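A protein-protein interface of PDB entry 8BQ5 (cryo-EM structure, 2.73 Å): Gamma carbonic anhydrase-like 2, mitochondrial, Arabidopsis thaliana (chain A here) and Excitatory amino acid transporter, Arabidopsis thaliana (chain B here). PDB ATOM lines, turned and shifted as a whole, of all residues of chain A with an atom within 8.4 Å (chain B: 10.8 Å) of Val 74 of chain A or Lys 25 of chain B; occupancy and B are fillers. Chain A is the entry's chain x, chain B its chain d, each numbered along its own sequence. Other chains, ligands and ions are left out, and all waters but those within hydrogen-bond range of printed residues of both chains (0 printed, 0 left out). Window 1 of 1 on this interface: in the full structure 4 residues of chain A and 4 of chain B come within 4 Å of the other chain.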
ATOM      1  N   LYS A  71     -16.270  34.020  34.298  1.00  0.00           N
ATOM      2  CA  LYS A  71     -16.988  34.125  33.035  1.00  0.00           C
ATOM      3  C   LYS A  71     -16.889  32.799  32.296  1.00  0.00           C
ATOM      4  O   LYS A  71     -15.796  32.397  31.884  1.00  0.00           O
ATOM      5  CB  LYS A  71     -16.420  35.261  32.186  1.00  0.00           C
ATOM      6  CG  LYS A  71     -17.325  35.727  31.060  1.00  0.00           C
ATOM      7  CD  LYS A  71     -16.841  37.051  30.492  1.00  0.00           C
ATOM      8  CE  LYS A  71     -15.880  36.839  29.334  1.00  0.00           C
ATOM      9  NZ  LYS A  71     -16.525  37.073  28.012  1.00  0.00           N
ATOM     10  N   VAL A  72     -18.023  32.131  32.120  1.00  0.00           N
ATOM     11  CA  VAL A  72     -18.078  30.828  31.470  1.00  0.00           C
ATOM     12  C   VAL A  72     -18.836  30.978  30.160  1.00  0.00           C
ATOM     13  O   VAL A  72     -19.955  31.501  30.140  1.00  0.00           O
ATOM     14  CB  VAL A  72     -18.744  29.773  32.371  1.00  0.00           C
ATOM     15  CG1 VAL A  72     -18.851  28.442  31.645  1.00  0.00           C
ATOM     16  CG2 VAL A  72     -17.963  29.620  33.656  1.00  0.00           C
ATOM     17  N   ALA A  73     -18.221  30.526  29.071  1.00  0.00           N
ATOM     18  CA  ALA A  73     -18.881  30.552  27.777  1.00  0.00           C
ATOM     19  C   ALA A  73     -20.087  29.622  27.773  1.00  0.00           C
ATOM     20  O   ALA A  73     -20.079  28.549  28.382  1.00  0.00           O
ATOM     21  CB  ALA A  73     -17.909  30.155  26.668  1.00  0.00           C
ATOM     22  N   VAL A  74     -21.133  30.048  27.062  1.00  0.00           N
ATOM     23  CA  VAL A  74     -22.388  29.310  27.023  1.00  0.00           C
ATOM     24  C   VAL A  74     -22.223  27.904  26.454  1.00  0.00           C
ATOM     25  O   VAL A  74     -23.023  27.017  26.771  1.00  0.00           O
ATOM     26  CB  VAL A  74     -23.430  30.124  26.230  1.00  0.00           C
ATOM     27  CG1 VAL A  74     -23.229  29.952  24.730  1.00  0.00           C
ATOM     28  CG2 VAL A  74     -24.832  29.726  26.637  1.00  0.00           C
ATOM     29  N   ASP A  75     -21.202  27.665  25.632  1.00  0.00           N
ATOM     30  CA  ASP A  75     -20.949  26.349  25.056  1.00  0.00           C
ATOM     31  C   ASP A  75     -19.689  25.696  25.624  1.00  0.00           C
ATOM     32  O   ASP A  75     -19.005  24.938  24.933  1.00  0.00           O
ATOM     33  CB  ASP A  75     -20.894  26.437  23.529  1.00  0.00           C
ATOM     34  CG  ASP A  75     -19.566  26.960  23.007  1.00  0.00           C
ATOM     35  OD1 ASP A  75     -18.788  27.530  23.796  1.00  0.00           O
ATOM     36  OD2 ASP A  75     -19.289  26.782  21.803  1.00  0.00           O
ATOM     37  N   ALA A  76     -19.371  25.978  26.882  1.00  0.00           N
ATOM     38  CA  ALA A  76     -18.251  25.356  27.569  1.00  0.00           C
ATOM     39  C   ALA A  76     -18.782  24.409  28.636  1.00  0.00           C
ATOM     40  O   ALA A  76     -19.838  24.656  29.224  1.00  0.00           O
ATOM     41  CB  ALA A  76     -17.336  26.406  28.203  1.00  0.00           C
ATOM     42  N   TYR A  77     -18.058  23.321  28.876  1.00  0.00           N
ATOM     43  CA  TYR A  77     -18.435  22.354  29.896  1.00  0.00           C
ATOM     44  C   TYR A  77     -17.596  22.574  31.149  1.00  0.00           C
ATOM     45  O   TYR A  77     -16.364  22.553  31.087  1.00  0.00           O
ATOM     46  CB  TYR A  77     -18.268  20.918  29.404  1.00  0.00           C
ATOM     47  CG  TYR A  77     -18.569  19.923  30.495  1.00  0.00           C
ATOM     48  CD1 TYR A  77     -19.839  19.834  31.044  1.00  0.00           C
ATOM     49  CD2 TYR A  77     -17.574  19.106  31.010  1.00  0.00           C
ATOM     50  CE1 TYR A  77     -20.117  18.944  32.055  1.00  0.00           C
ATOM     51  CE2 TYR A  77     -17.843  18.212  32.024  1.00  0.00           C
ATOM     52  CZ  TYR A  77     -19.116  18.135  32.542  1.00  0.00           C
ATOM     53  OH  TYR A  77     -19.393  17.245  33.552  1.00  0.00           O
ATOM     54  N   VAL A  90     -13.465  31.256  31.001  1.00  0.00           N
ATOM     55  CA  VAL A  90     -13.496  29.948  30.360  1.00  0.00           C
ATOM     56  C   VAL A  90     -14.181  30.141  29.012  1.00  0.00           C
ATOM     57  O   VAL A  90     -15.375  30.459  28.954  1.00  0.00           O
ATOM     58  CB  VAL A  90     -14.220  28.912  31.233  1.00  0.00           C
ATOM     59  CG1 VAL A  90     -14.750  27.764  30.410  1.00  0.00           C
ATOM     60  CG2 VAL A  90     -13.290  28.403  32.325  1.00  0.00           C
ATOM     61  N   TRP A  91     -13.425  29.964  27.929  1.00  0.00           N
ATOM     62  CA  TRP A  91     -13.872  30.383  26.610  1.00  0.00           C
ATOM     63  C   TRP A  91     -14.648  29.279  25.896  1.00  0.00           C
ATOM     64  O   TRP A  91     -14.883  28.192  26.428  1.00  0.00           O
ATOM     65  CB  TRP A  91     -12.686  30.830  25.759  1.00  0.00           C
ATOM     66  CG  TRP A  91     -12.223  32.210  26.067  1.00  0.00           C
ATOM     67  CD1 TRP A  91     -11.071  32.563  26.701  1.00  0.00           C
ATOM     68  CD2 TRP A  91     -12.912  33.430  25.777  1.00  0.00           C
ATOM     69  NE1 TRP A  91     -10.991  33.927  26.810  1.00  0.00           N
ATOM     70  CE2 TRP A  91     -12.111  34.484  26.252  1.00  0.00           C
ATOM     71  CE3 TRP A  91     -14.127  33.733  25.155  1.00  0.00           C
ATOM     72  CZ2 TRP A  91     -12.484  35.818  26.129  1.00  0.00           C
ATOM     73  CZ3 TRP A  91     -14.495  35.058  25.032  1.00  0.00           C
ATOM     74  CH2 TRP A  91     -13.676  36.084  25.516  1.00  0.00           C
ATOM     75  N   ASP A  92     -15.035  29.571  24.657  1.00  0.00           N
ATOM     76  CA  ASP A  92     -15.916  28.692  23.900  1.00  0.00           C
ATOM     77  C   ASP A  92     -15.234  27.371  23.571  1.00  0.00           C
ATOM     78  O   ASP A  92     -14.074  27.334  23.157  1.00  0.00           O
ATOM     79  CB  ASP A  92     -16.362  29.385  22.614  1.00  0.00           C
ATOM     80  CG  ASP A  92     -17.114  30.671  22.880  1.00  0.00           C
ATOM     81  OD1 ASP A  92     -18.280  30.780  22.449  1.00  0.00           O
ATOM     82  OD2 ASP A  92     -16.540  31.570  23.532  1.00  0.00           O
ATOM     83  N   GLY A  93     -15.971  26.278  23.755  1.00  0.00           N
ATOM     84  CA  GLY A  93     -15.470  24.960  23.435  1.00  0.00           C
ATOM     85  C   GLY A  93     -14.493  24.388  24.433  1.00  0.00           C
ATOM     86  O   GLY A  93     -13.965  23.294  24.199  1.00  0.00           O
ATOM     87  N   SER A  94     -14.235  25.083  25.533  1.00  0.00           N
ATOM     88  CA  SER A  94     -13.305  24.606  26.538  1.00  0.00           C
ATOM     89  C   SER A  94     -14.039  23.778  27.592  1.00  0.00           C
ATOM     90  O   SER A  94     -15.253  23.884  27.773  1.00  0.00           O
ATOM     91  CB  SER A  94     -12.572  25.781  27.179  1.00  0.00           C
ATOM     92  OG  SER A  94     -13.463  26.593  27.910  1.00  0.00           O
ATOM     93  N   PHE A 113      -9.752  28.952  23.592  1.00  0.00           N
ATOM     94  CA  PHE A 113     -10.693  28.256  22.724  1.00  0.00           C
ATOM     95  C   PHE A 113     -10.343  26.777  22.602  1.00  0.00           C
ATOM     96  O   PHE A 113      -9.214  26.420  22.260  1.00  0.00           O
ATOM     97  CB  PHE A 113     -10.698  28.917  21.345  1.00  0.00           C
ATOM     98  CG  PHE A 113     -11.522  28.194  20.322  1.00  0.00           C
ATOM     99  CD1 PHE A 113     -12.898  28.345  20.291  1.00  0.00           C
ATOM    100  CD2 PHE A 113     -10.921  27.369  19.387  1.00  0.00           C
ATOM    101  CE1 PHE A 113     -13.657  27.683  19.350  1.00  0.00           C
ATOM    102  CE2 PHE A 113     -11.677  26.704  18.444  1.00  0.00           C
ATOM    103  CZ  PHE A 113     -13.045  26.862  18.425  1.00  0.00           C
ATOM    104  N   CYS A 114     -11.321  25.920  22.896  1.00  0.00           N
ATOM    105  CA  CYS A 114     -11.203  24.472  22.707  1.00  0.00           C
ATOM    106  C   CYS A 114     -10.082  23.860  23.548  1.00  0.00           C
ATOM    107  O   CYS A 114      -9.568  22.789  23.224  1.00  0.00           O
ATOM    108  CB  CYS A 114     -11.009  24.127  21.228  1.00  0.00           C
ATOM    109  SG  CYS A 114     -10.936  22.361  20.868  1.00  0.00           S
ATOM    110  N   ASN A 225     -12.916  17.905  23.423  1.00  0.00           N
ATOM    111  CA  ASN A 225     -14.115  18.741  23.381  1.00  0.00           C
ATOM    112  C   ASN A 225     -15.340  17.929  22.963  1.00  0.00           C
ATOM    113  O   ASN A 225     -16.435  18.096  23.521  1.00  0.00           O
ATOM    114  CB  ASN A 225     -13.887  19.923  22.437  1.00  0.00           C
ATOM    115  CG  ASN A 225     -15.176  20.487  21.879  1.00  0.00           C
ATOM    116  OD1 ASN A 225     -15.807  21.350  22.489  1.00  0.00           O
ATOM    117  ND2 ASN A 225     -15.566  20.015  20.703  1.00  0.00           N
ATOM    118  N   PHE A 232     -21.939  17.673  28.665  1.00  0.00           N
ATOM    119  CA  PHE A 232     -22.728  18.899  28.619  1.00  0.00           C
ATOM    120  C   PHE A 232     -24.198  18.595  28.373  1.00  0.00           C
ATOM    121  O   PHE A 232     -25.080  19.211  28.983  1.00  0.00           O
ATOM    122  CB  PHE A 232     -22.187  19.823  27.528  1.00  0.00           C
ATOM    123  CG  PHE A 232     -22.806  21.190  27.523  1.00  0.00           C
ATOM    124  CD1 PHE A 232     -23.982  21.433  26.834  1.00  0.00           C
ATOM    125  CD2 PHE A 232     -22.201  22.237  28.191  1.00  0.00           C
ATOM    126  CE1 PHE A 232     -24.551  22.690  26.826  1.00  0.00           C
ATOM    127  CE2 PHE A 232     -22.762  23.497  28.184  1.00  0.00           C
ATOM    128  CZ  PHE A 232     -23.939  23.723  27.500  1.00  0.00           C
ATOM    129  N   GLN B  17     -36.081  28.814  14.385  1.00  0.00           N
ATOM    130  CA  GLN B  17     -35.815  28.665  15.838  1.00  0.00           C
ATOM    131  C   GLN B  17     -34.476  27.946  16.061  1.00  0.00           C
ATOM    132  O   GLN B  17     -33.684  28.438  16.871  1.00  0.00           O
ATOM    133  CB  GLN B  17     -36.987  27.950  16.515  1.00  0.00           C
ATOM    134  CG  GLN B  17     -36.768  27.661  17.993  1.00  0.00           C
ATOM    135  CD  GLN B  17     -36.457  28.868  18.847  1.00  0.00           C
ATOM    136  OE1 GLN B  17     -36.899  29.983  18.582  1.00  0.00           O
ATOM    137  NE2 GLN B  17     -35.697  28.641  19.903  1.00  0.00           N
ATOM    138  N   MET B  18     -34.226  26.849  15.346  1.00  0.00           N
ATOM    139  CA  MET B  18     -32.955  26.092  15.484  1.00  0.00           C
ATOM    140  C   MET B  18     -31.792  26.935  14.944  1.00  0.00           C
ATOM    141  O   MET B  18     -30.723  26.878  15.547  1.00  0.00           O
ATOM    142  CB  MET B  18     -33.064  24.755  14.745  1.00  0.00           C
ATOM    143  CG  MET B  18     -34.171  23.871  15.288  1.00  0.00           C
ATOM    144  SD  MET B  18     -34.480  22.360  14.338  1.00  0.00           S
ATOM    145  CE  MET B  18     -32.973  21.450  14.668  1.00  0.00           C
ATOM    146  N   TYR B  19     -31.999  27.680  13.857  1.00  0.00           N
ATOM    147  CA  TYR B  19     -30.967  28.593  13.298  1.00  0.00           C
ATOM    148  C   TYR B  19     -30.673  29.681  14.334  1.00  0.00           C
ATOM    149  O   TYR B  19     -29.502  29.958  14.584  1.00  0.00           O
ATOM    150  CB  TYR B  19     -31.487  29.150  11.970  1.00  0.00           C
ATOM    151  CG  TYR B  19     -30.503  29.757  11.007  1.00  0.00           C
ATOM    152  CD1 TYR B  19     -29.171  29.944  11.334  1.00  0.00           C
ATOM    153  CD2 TYR B  19     -30.922  30.153   9.749  1.00  0.00           C
ATOM    154  CE1 TYR B  19     -28.284  30.510  10.436  1.00  0.00           C
ATOM    155  CE2 TYR B  19     -30.047  30.715   8.836  1.00  0.00           C
ATOM    156  CZ  TYR B  19     -28.724  30.897   9.183  1.00  0.00           C
ATOM    157  OH  TYR B  19     -27.857  31.447   8.286  1.00  0.00           O
ATOM    158  N   SER B  20     -31.714  30.252  14.939  1.00  0.00           N
ATOM    159  CA  SER B  20     -31.557  31.284  16.000  1.00  0.00           C
ATOM    160  C   SER B  20     -30.814  30.704  17.210  1.00  0.00           C
ATOM    161  O   SER B  20     -29.917  31.382  17.706  1.00  0.00           O
ATOM    162  CB  SER B  20     -32.899  31.838  16.388  1.00  0.00           C
ATOM    163  OG  SER B  20     -32.793  32.708  17.502  1.00  0.00           O
ATOM    164  N   ASN B  21     -31.145  29.480  17.623  1.00  0.00           N
ATOM    165  CA  ASN B  21     -30.431  28.811  18.745  1.00  0.00           C
ATOM    166  C   ASN B  21     -28.966  28.599  18.371  1.00  0.00           C
ATOM    167  O   ASN B  21     -28.113  28.876  19.216  1.00  0.00           O
ATOM    168  CB  ASN B  21     -31.077  27.477  19.117  1.00  0.00           C
ATOM    169  CG  ASN B  21     -32.229  27.625  20.087  1.00  0.00           C
ATOM    170  OD1 ASN B  21     -32.332  28.623  20.790  1.00  0.00           O
ATOM    171  ND2 ASN B  21     -33.096  26.631  20.138  1.00  0.00           N
ATOM    172  N   ALA B  22     -28.697  28.142  17.147  1.00  0.00           N
ATOM    173  CA  ALA B  22     -27.316  27.866  16.692  1.00  0.00           C
ATOM    174  C   ALA B  22     -26.496  29.161  16.583  1.00  0.00           C
ATOM    175  O   ALA B  22     -25.315  29.125  16.958  1.00  0.00           O
ATOM    176  CB  ALA B  22     -27.363  27.124  15.379  1.00  0.00           C
ATOM    177  N   LEU B  23     -27.095  30.256  16.103  1.00  0.00           N
ATOM    178  CA  LEU B  23     -26.392  31.564  16.025  1.00  0.00           C
ATOM    179  C   LEU B  23     -25.980  32.026  17.424  1.00  0.00           C
ATOM    180  O   LEU B  23     -24.970  32.730  17.524  1.00  0.00           O
ATOM    181  CB  LEU B  23     -27.289  32.599  15.335  1.00  0.00           C
ATOM    182  CG  LEU B  23     -27.403  32.459  13.820  1.00  0.00           C
ATOM    183  CD1 LEU B  23     -28.560  33.284  13.280  1.00  0.00           C
ATOM    184  CD2 LEU B  23     -26.100  32.841  13.137  1.00  0.00           C
ATOM    185  N   ARG B  24     -26.737  31.648  18.456  1.00  0.00           N
ATOM    186  CA  ARG B  24     -26.391  32.023  19.818  1.00  0.00           C
ATOM    187  C   ARG B  24     -25.514  30.985  20.499  1.00  0.00           C
ATOM    188  O   ARG B  24     -25.254  31.103  21.700  1.00  0.00           O
ATOM    189  CB  ARG B  24     -27.663  32.252  20.633  1.00  0.00           C
ATOM    190  CG  ARG B  24     -28.626  33.211  19.971  1.00  0.00           C
ATOM    191  CD  ARG B  24     -30.010  33.113  20.569  1.00  0.00           C
ATOM    192  NE  ARG B  24     -30.024  33.542  21.961  1.00  0.00           N
ATOM    193  CZ  ARG B  24     -30.948  33.190  22.844  1.00  0.00           C
ATOM    194  NH1 ARG B  24     -31.963  32.410  22.508  1.00  0.00           N
ATOM    195  NH2 ARG B  24     -30.857  33.639  24.090  1.00  0.00           N
ATOM    196  N   LYS B  25     -25.067  29.972  19.754  1.00  0.00           N
ATOM    197  CA  LYS B  25     -24.247  28.878  20.274  1.00  0.00           C
ATOM    198  C   LYS B  25     -24.973  28.081  21.350  1.00  0.00           C
ATOM    199  O   LYS B  25     -24.351  27.536  22.263  1.00  0.00           O
ATOM    200  CB  LYS B  25     -22.903  29.385  20.800  1.00  0.00           C
ATOM    201  CG  LYS B  25     -21.987  29.892  19.716  1.00  0.00           C
ATOM    202  CD  LYS B  25     -20.868  28.907  19.468  1.00  0.00           C
ATOM    203  CE  LYS B  25     -19.530  29.601  19.449  1.00  0.00           C
ATOM    204  NZ  LYS B  25     -18.412  28.623  19.521  1.00  0.00           N
ATOM    205  N   LEU B  26     -26.283  28.001  21.248  1.00  0.00           N
ATOM    206  CA  LEU B  26     -27.076  27.189  22.150  1.00  0.00           C
ATOM    207  C   LEU B  26     -27.386  25.841  21.520  1.00  0.00           C
ATOM    208  O   LEU B  26     -27.254  25.663  20.306  1.00  0.00           O
ATOM    209  CB  LEU B  26     -28.383  27.899  22.504  1.00  0.00           C
ATOM    210  CG  LEU B  26     -28.276  29.194  23.304  1.00  0.00           C
ATOM    211  CD1 LEU B  26     -29.624  29.882  23.344  1.00  0.00           C
ATOM    212  CD2 LEU B  26     -27.770  28.914  24.704  1.00  0.00           C
ATOM    213  N   PRO B  27     -27.789  24.859  22.325  1.00  0.00           N
ATOM    214  CA  PRO B  27     -28.289  23.602  21.756  1.00  0.00           C
ATOM    215  C   PRO B  27     -29.495  23.852  20.862  1.00  0.00           C
ATOM    216  O   PRO B  27     -30.267  24.788  21.073  1.00  0.00           O
ATOM    217  CB  PRO B  27     -28.672  22.778  22.989  1.00  0.00           C
ATOM    218  CG  PRO B  27     -27.878  23.344  24.104  1.00  0.00           C
ATOM    219  CD  PRO B  27     -27.556  24.770  23.777  1.00  0.00           C
ATOM    220  N   TYR B  28     -29.641  23.000  19.842  1.00  0.00           N
ATOM    221  CA  TYR B  28     -30.716  23.174  18.869  1.00  0.00           C
ATOM    222  C   TYR B  28     -32.080  23.245  19.543  1.00  0.00           C
ATOM    223  O   TYR B  28     -32.865  24.162  19.281  1.00  0.00           O
ATOM    224  CB  TYR B  28     -30.703  22.032  17.854  1.00  0.00           C
ATOM    225  CG  TYR B  28     -29.737  22.218  16.712  1.00  0.00           C
ATOM    226  CD1 TYR B  28     -29.742  23.377  15.950  1.00  0.00           C
ATOM    227  CD2 TYR B  28     -28.824  21.226  16.393  1.00  0.00           C
ATOM    228  CE1 TYR B  28     -28.858  23.543  14.904  1.00  0.00           C
ATOM    229  CE2 TYR B  28     -27.939  21.381  15.352  1.00  0.00           C
ATOM    230  CZ  TYR B  28     -27.958  22.538  14.612  1.00  0.00           C
ATOM    231  OH  TYR B  28     -27.072  22.685  13.574  1.00  0.00           O
ATOM    232  N   MET B  29     -32.386  22.273  20.399  1.00  0.00           N
ATOM    233  CA  MET B  29     -33.670  22.188  21.084  1.00  0.00           C
ATOM    234  C   MET B  29     -33.618  22.799  22.481  1.00  0.00           C
ATOM    235  O   MET B  29     -34.050  22.183  23.455  1.00  0.00           O
ATOM    236  CB  MET B  29     -34.128  20.736  21.162  1.00  0.00           C
ATOM    237  CG  MET B  29     -33.952  19.981  19.862  1.00  0.00           C
ATOM    238  SD  MET B  29     -34.885  20.748  18.528  1.00  0.00           S
ATOM    239  CE  MET B  29     -36.555  20.385  19.057  1.00  0.00           C
ATOM    240  N   ARG B  30     -33.117  24.030  22.595  1.00  0.00           N
ATOM    241  CA  ARG B  30     -32.942  24.626  23.916  1.00  0.00           C
ATOM    242  C   ARG B  30     -34.289  24.908  24.577  1.00  0.00           C
ATOM    243  O   ARG B  30     -34.511  24.528  25.728  1.00  0.00           O
ATOM    244  CB  ARG B  30     -32.081  25.889  23.813  1.00  0.00           C
ATOM    245  CG  ARG B  30     -32.160  26.880  24.985  1.00  0.00           C
ATOM    246  CD  ARG B  30     -32.008  26.267  26.385  1.00  0.00           C
ATOM    247  NE  ARG B  30     -30.932  25.291  26.503  1.00  0.00           N
ATOM    248  CZ  ARG B  30     -29.809  25.494  27.179  1.00  0.00           C
ATOM    249  NH1 ARG B  30     -29.565  26.642  27.787  1.00  0.00           N
ATOM    250  NH2 ARG B  30     -28.909  24.517  27.248  1.00  0.00           N
ATOM    251  N   HIS B  31     -35.212  25.547  23.864  1.00  0.00           N
ATOM    252  CA  HIS B  31     -36.542  25.836  24.403  1.00  0.00           C
ATOM    253  C   HIS B  31     -37.581  25.271  23.442  1.00  0.00           C
ATOM    254  O   HIS B  31     -38.091  25.992  22.572  1.00  0.00           O
ATOM    255  CB  HIS B  31     -36.738  27.334  24.618  1.00  0.00           C
ATOM    256  CG  HIS B  31     -36.078  27.865  25.853  1.00  0.00           C
ATOM    257  ND1 HIS B  31     -36.023  29.210  26.147  1.00  0.00           N
ATOM    258  CD2 HIS B  31     -35.449  27.232  26.872  1.00  0.00           C
ATOM    259  CE1 HIS B  31     -35.386  29.384  27.291  1.00  0.00           C
ATOM    260  NE2 HIS B  31     -35.029  28.200  27.752  1.00  0.00           N
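The side-chain amino group (NZ) of Lys 25 of chain B is in salt-bridge range of the side-chain carboxylate (OD1) of Asp 92 of chain A (3.6 Å).
The side-chain carboxylate (OD2) of Asp 75 of chain A is in salt-bridge range of the side-chain amino group (NZ) of Lys 25 of chain B, at 3.1 Å.
Val 74 of chain A touches just these residues of chain B: Arg 24 (3.8 Å), Lys 25 (3.6 Å) and Leu 26 (3.6 Å).
Of chain B, only Lys 25 comes within 4 Å of Asp 75 of chain A.
Asp 92 of chain A touches just one residue of chain B: Lys 25 (3.5 Å).
Met 18 of chain B touches none of the printed residues of chain A.
Printed residues of chain A within 4 Å of Arg 24 of chain B: Val 74.
Of chain A, only Val 74 (3.6 Å), Asp 75 (3.1 Å) and Asp 92 (3.5 Å) come within 4 Å of Lys 25 of chain B.
Of the printed residues of chain A, Leu 26 of chain B touches Val 74 (3.6 Å).
The nearest residue of chain B that does not touch Val 74 of chain A is Arg 30 of chain B (5.8 Å).
The nearest residue of chain A that does not touch Lys 25 of chain B is Phe 113 of chain A (4.9 Å).
The backbone carbonyl oxygen (O) of Asp 92 of chain A lies within hydrogen-bond range of the backbone NH (N) of Cys 114 of chain A, at 3.1 Å.
OD1 of Asp 75 of chain A is in hydrogen-bond range of N of Gly 93 of chain A, at 3.1 Å.
O of Asn 21 of chain B sits at hydrogen-bond distance from N of Leu 26 of chain B (2.9 Å).
Of the 16 printed residues of chain A, 3 touch a printed residue of chain B.
Printed residues of chain A that touch a printed residue of chain B: Val 74, Asp 75 and Asp 92.
Hydrophobic or aromatic side chains of chain A within 4 Å of the printed part of chain B: Val 74.
Among the printed residues, 5 pairs touch across the chains.
Among the printed residues, Asp or Glu carboxylates within 4 Å of a Lys or Arg side-chain nitrogen of the other chain: Asp 75 of chain A with Lys 25 of chain B (3.1 Å) and Asp 92 of chain A with Lys 25 of chain B (3.6 Å).
O of Arg 24 of chain B touches CG1 of Val 74 of chain A (3.8 Å).
O of Lys 25 of chain B touches CG1 of Val 74 of chain A, at 3.6 Å.
CG2 of Val 74 of chain A touches CD2 of Leu 26 of chain B (3.6 Å).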
